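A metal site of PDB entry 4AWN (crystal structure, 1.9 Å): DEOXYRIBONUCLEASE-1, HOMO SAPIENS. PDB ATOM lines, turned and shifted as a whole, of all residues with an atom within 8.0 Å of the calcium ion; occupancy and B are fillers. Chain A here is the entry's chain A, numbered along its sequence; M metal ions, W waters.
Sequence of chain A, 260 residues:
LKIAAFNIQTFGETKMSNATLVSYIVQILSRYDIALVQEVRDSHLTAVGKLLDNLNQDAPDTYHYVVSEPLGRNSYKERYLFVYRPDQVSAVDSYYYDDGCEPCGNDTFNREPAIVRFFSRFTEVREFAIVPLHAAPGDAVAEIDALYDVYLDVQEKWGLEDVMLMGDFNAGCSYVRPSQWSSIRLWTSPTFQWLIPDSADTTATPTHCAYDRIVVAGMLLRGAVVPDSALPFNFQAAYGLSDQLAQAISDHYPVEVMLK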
ATOM      1  N   ALA A 200      19.057 -14.217   7.820  1.00  0.00           N
ATOM      2  CA  ALA A 200      19.723 -15.079   6.838  1.00  0.00           C
ATOM      3  C   ALA A 200      19.857 -16.492   7.378  1.00  0.00           C
ATOM      4  O   ALA A 200      19.952 -16.691   8.582  1.00  0.00           O
ATOM      5  CB  ALA A 200      21.088 -14.520   6.484  1.00  0.00           C
ATOM      6  N   ASP A 201      19.814 -17.473   6.472  1.00  0.00           N
ATOM      7  CA  ASP A 201      20.177 -18.851   6.809  1.00  0.00           C
ATOM      8  C   ASP A 201      21.520 -19.161   6.148  1.00  0.00           C
ATOM      9  O   ASP A 201      21.580 -19.283   4.905  1.00  0.00           O
ATOM     10  CB  ASP A 201      19.130 -19.858   6.297  1.00  0.00           C
ATOM     11  CG  ASP A 201      19.529 -21.306   6.566  1.00  0.00           C
ATOM     12  OD1 ASP A 201      20.369 -21.557   7.464  1.00  0.00           O
ATOM     13  OD2 ASP A 201      18.999 -22.213   5.904  1.00  0.00           O
ATOM     14  N   THR A 202      22.589 -19.275   6.927  1.00  0.00           N
ATOM     15  CA  THR A 202      23.901 -19.604   6.327  1.00  0.00           C
ATOM     16  C   THR A 202      24.369 -21.037   6.694  1.00  0.00           C
ATOM     17  O   THR A 202      25.570 -21.350   6.561  1.00  0.00           O
ATOM     18  CB  THR A 202      24.990 -18.578   6.728  1.00  0.00           C
ATOM     19  OG1 THR A 202      25.308 -18.764   8.106  1.00  0.00           O
ATOM     20  CG2 THR A 202      24.518 -17.119   6.494  1.00  0.00           C
ATOM     21  N   THR A 203      23.441 -21.876   7.156  1.00  0.00           N
ATOM     22  CA  THR A 203      23.772 -23.275   7.455  1.00  0.00           C
ATOM     23  C   THR A 203      23.230 -24.189   6.361  1.00  0.00           C
ATOM     24  O   THR A 203      22.100 -24.020   5.899  1.00  0.00           O
ATOM     25  CB  THR A 203      23.284 -23.755   8.829  1.00  0.00           C
ATOM     26  OG1 THR A 203      21.861 -23.915   8.822  1.00  0.00           O
ATOM     27  CG2 THR A 203      23.651 -22.774   9.919  1.00  0.00           C
ATOM     28  N   ALA A 204      24.054 -25.155   5.951  1.00  0.00           N
ATOM     29  CA  ALA A 204      23.665 -26.154   4.980  1.00  0.00           C
ATOM     30  C   ALA A 204      22.788 -27.233   5.573  1.00  0.00           C
ATOM     31  O   ALA A 204      22.207 -28.049   4.854  1.00  0.00           O
ATOM     32  CB  ALA A 204      24.902 -26.774   4.365  1.00  0.00           C
ATOM     33  N   THR A 205      22.725 -27.261   6.899  1.00  0.00           N
ATOM     34  CA  THR A 205      21.882 -28.200   7.641  1.00  0.00           C
ATOM     35  C   THR A 205      20.481 -27.576   7.814  1.00  0.00           C
ATOM     36  O   THR A 205      20.280 -26.385   7.497  1.00  0.00           O
ATOM     37  CB  THR A 205      22.510 -28.451   9.026  1.00  0.00           C
ATOM     38  OG1 THR A 205      22.401 -27.258   9.810  1.00  0.00           O
ATOM     39  CG2 THR A 205      23.964 -28.827   8.888  1.00  0.00           C
ATOM     40  N   PRO A 206      19.498 -28.369   8.333  1.00  0.00           N
ATOM     41  CA  PRO A 206      18.146 -27.826   8.476  1.00  0.00           C
ATOM     42  C   PRO A 206      17.928 -26.701   9.512  1.00  0.00           C
ATOM     43  O   PRO A 206      16.837 -26.161   9.560  1.00  0.00           O
ATOM     44  CB  PRO A 206      17.291 -29.049   8.836  1.00  0.00           C
ATOM     45  CG  PRO A 206      18.274 -30.070   9.353  1.00  0.00           C
ATOM     46  CD  PRO A 206      19.545 -29.820   8.581  1.00  0.00           C
ATOM     47  N   THR A 207      18.939 -26.344  10.310  1.00  0.00           N
ATOM     48  CA  THR A 207      18.800 -25.177  11.188  1.00  0.00           C
ATOM     49  C   THR A 207      18.683 -23.909  10.346  1.00  0.00           C
ATOM     50  O   THR A 207      19.096 -23.893   9.192  1.00  0.00           O
ATOM     51  CB  THR A 207      20.000 -24.970  12.163  1.00  0.00           C
ATOM     52  OG1 THR A 207      21.192 -24.689  11.414  1.00  0.00           O
ATOM     53  CG2 THR A 207      20.237 -26.188  13.083  1.00  0.00           C
ATOM     54  N   HIS A 208      18.173 -22.839  10.912  1.00  0.00           N
ATOM     55  CA  HIS A 208      18.091 -21.576  10.238  1.00  0.00           C
ATOM     56  C   HIS A 208      18.837 -20.547  11.060  1.00  0.00           C
ATOM     57  O   HIS A 208      18.311 -20.015  11.996  1.00  0.00           O
ATOM     58  CB  HIS A 208      16.645 -21.187  10.009  1.00  0.00           C
ATOM     59  CG  HIS A 208      16.461 -19.951   9.190  1.00  0.00           C
ATOM     60  ND1 HIS A 208      15.972 -19.969   7.971  1.00  0.00           N
ATOM     61  CD2 HIS A 208      16.725 -18.642   9.479  1.00  0.00           C
ATOM     62  CE1 HIS A 208      15.949 -18.717   7.497  1.00  0.00           C
ATOM     63  NE2 HIS A 208      16.419 -17.921   8.418  1.00  0.00           N
ATOM     64  N   CYS A 209      20.098 -20.323  10.729  1.00  0.00           N
ATOM     65  CA  CYS A 209      20.981 -19.494  11.558  1.00  0.00           C
ATOM     66  C   CYS A 209      21.806 -18.554  10.722  1.00  0.00           C
ATOM     67  O   CYS A 209      22.349 -18.953   9.696  1.00  0.00           O
ATOM     68  CB  CYS A 209      21.907 -20.363  12.426  1.00  0.00           C
ATOM     69  SG  CYS A 209      21.028 -21.548  13.512  1.00  0.00           S
ATOM     70  N   ASN A 234      23.340 -20.689  -1.373  1.00  0.00           N
ATOM     71  CA  ASN A 234      22.843 -22.044  -1.100  1.00  0.00           C
ATOM     72  C   ASN A 234      23.257 -22.980  -2.252  1.00  0.00           C
ATOM     73  O   ASN A 234      22.551 -23.095  -3.268  1.00  0.00           O
ATOM     74  CB  ASN A 234      21.297 -21.998  -0.867  1.00  0.00           C
ATOM     75  CG  ASN A 234      20.699 -23.358  -0.485  1.00  0.00           C
ATOM     76  OD1 ASN A 234      21.297 -24.418  -0.728  1.00  0.00           O
ATOM     77  ND2 ASN A 234      19.489 -23.340   0.098  1.00  0.00           N
ATOM     78  N   GLN A 236      23.370 -26.153  -2.243  1.00  0.00           N
ATOM     79  CA  GLN A 236      22.491 -27.327  -2.359  1.00  0.00           C
ATOM     80  C   GLN A 236      21.396 -27.080  -3.400  1.00  0.00           C
ATOM     81  O   GLN A 236      21.249 -27.858  -4.333  1.00  0.00           O
ATOM     82  CB  GLN A 236      21.865 -27.770  -1.030  1.00  0.00           C
ATOM     83  CG  GLN A 236      20.951 -28.991  -1.275  1.00  0.00           C
ATOM     84  CD  GLN A 236      20.296 -29.599  -0.050  1.00  0.00           C
ATOM     85  OE1 GLN A 236      20.496 -29.164   1.082  1.00  0.00           O
ATOM     86  NE2 GLN A 236      19.477 -30.613  -0.301  1.00  0.00           N
ATOM     87  N   GLN A 247      25.702 -31.575   2.664  1.00  0.00           N
ATOM     88  CA  GLN A 247      26.235 -31.518   4.004  1.00  0.00           C
ATOM     89  C   GLN A 247      27.627 -32.146   4.089  1.00  0.00           C
ATOM     90  O   GLN A 247      28.415 -31.802   4.975  1.00  0.00           O
ATOM     91  CB  GLN A 247      25.253 -32.170   4.974  1.00  0.00           C
ATOM     92  CG  GLN A 247      24.039 -31.270   5.307  1.00  0.00           C
ATOM     93  CD  GLN A 247      23.049 -31.927   6.273  1.00  0.00           C
ATOM     94  OE1 GLN A 247      21.838 -31.767   6.147  1.00  0.00           O
ATOM     95  NE2 GLN A 247      23.569 -32.678   7.216  1.00  0.00           N
ATOM     96  N   ASP A 251      28.794 -27.916   6.457  1.00  0.00           N
ATOM     97  CA  ASP A 251      27.568 -27.572   7.172  1.00  0.00           C
ATOM     98  C   ASP A 251      27.207 -26.109   7.040  1.00  0.00           C
ATOM     99  O   ASP A 251      26.199 -25.659   7.619  1.00  0.00           O
ATOM    100  CB  ASP A 251      27.645 -27.970   8.656  1.00  0.00           C
ATOM    101  CG  ASP A 251      28.803 -27.315   9.413  1.00  0.00           C
ATOM    102  OD1 ASP A 251      29.921 -27.218   8.856  1.00  0.00           O
ATOM    103  OD2 ASP A 251      28.612 -26.962  10.598  1.00  0.00           O
ATOM    104  N   HIS A 252      28.017 -25.333   6.303  1.00  0.00           N
ATOM    105  CA  HIS A 252      27.747 -23.911   6.109  1.00  0.00           C
ATOM    106  C   HIS A 252      27.588 -23.586   4.649  1.00  0.00           C
ATOM    107  O   HIS A 252      28.168 -24.247   3.811  1.00  0.00           O
ATOM    108  CB  HIS A 252      28.932 -23.036   6.625  1.00  0.00           C
ATOM    109  CG  HIS A 252      29.080 -23.023   8.111  1.00  0.00           C
ATOM    110  ND1 HIS A 252      28.592 -22.003   8.901  1.00  0.00           N
ATOM    111  CD2 HIS A 252      29.675 -23.907   8.955  1.00  0.00           C
ATOM    112  CE1 HIS A 252      28.887 -22.250  10.165  1.00  0.00           C
ATOM    113  NE2 HIS A 252      29.542 -23.400  10.223  1.00  0.00           N
ATOM    114  N   TYR A 253      26.851 -22.535   4.338  1.00  0.00           N
ATOM    115  CA  TYR A 253      26.912 -21.942   3.009  1.00  0.00           C
ATOM    116  C   TYR A 253      27.952 -20.811   3.027  1.00  0.00           C
ATOM    117  O   TYR A 253      28.123 -20.155   4.057  1.00  0.00           O
ATOM    118  CB  TYR A 253      25.579 -21.315   2.599  1.00  0.00           C
ATOM    119  CG  TYR A 253      24.403 -22.272   2.550  1.00  0.00           C
ATOM    120  CD1 TYR A 253      24.544 -23.561   2.023  1.00  0.00           C
ATOM    121  CD2 TYR A 253      23.152 -21.884   3.007  1.00  0.00           C
ATOM    122  CE1 TYR A 253      23.459 -24.449   1.964  1.00  0.00           C
ATOM    123  CE2 TYR A 253      22.043 -22.793   2.969  1.00  0.00           C
ATOM    124  CZ  TYR A 253      22.224 -24.050   2.451  1.00  0.00           C
ATOM    125  OH  TYR A 253      21.163 -24.933   2.414  1.00  0.00           O
HETATM  126 CA    CA M   1      19.933 -24.121   7.019  1.00  0.00          CA
HETATM  127  O   HOH W   1      19.575 -25.016   4.748  1.00  0.00           O
HETATM  128  O   HOH W   2      17.524 -24.821   6.798  1.00  0.00           O
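Within 4 Å of the calcium ion: Asp 201, Thr 203, Thr 205 and Thr 207. The nearest printed residue that does not touch the calcium ion is Pro 206 (4.1 Å).
The side-chain hydroxyl of Thr 205 is in hydrogen-bond range of the side-chain hydroxyl of Thr 207 (3.3 Å). OG1 of Thr 207 lies within hydrogen-bond range of SG of Cys 209 (3.8 Å).
The calcium ion is bound by the backbone carbonyl oxygen (O) of Thr 205, the backbone carbonyl oxygen (O) of Thr 207, the side-chain carboxylate (OD2) of Asp 201, the backbone carbonyl oxygen (O) of Thr 203, water W1, water W2, the side-chain carboxylate (OD1) of Asp 201 and the side-chain hydroxyl (OG1) of Thr 203. The calcium ion has eight donor atoms within binding distance.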
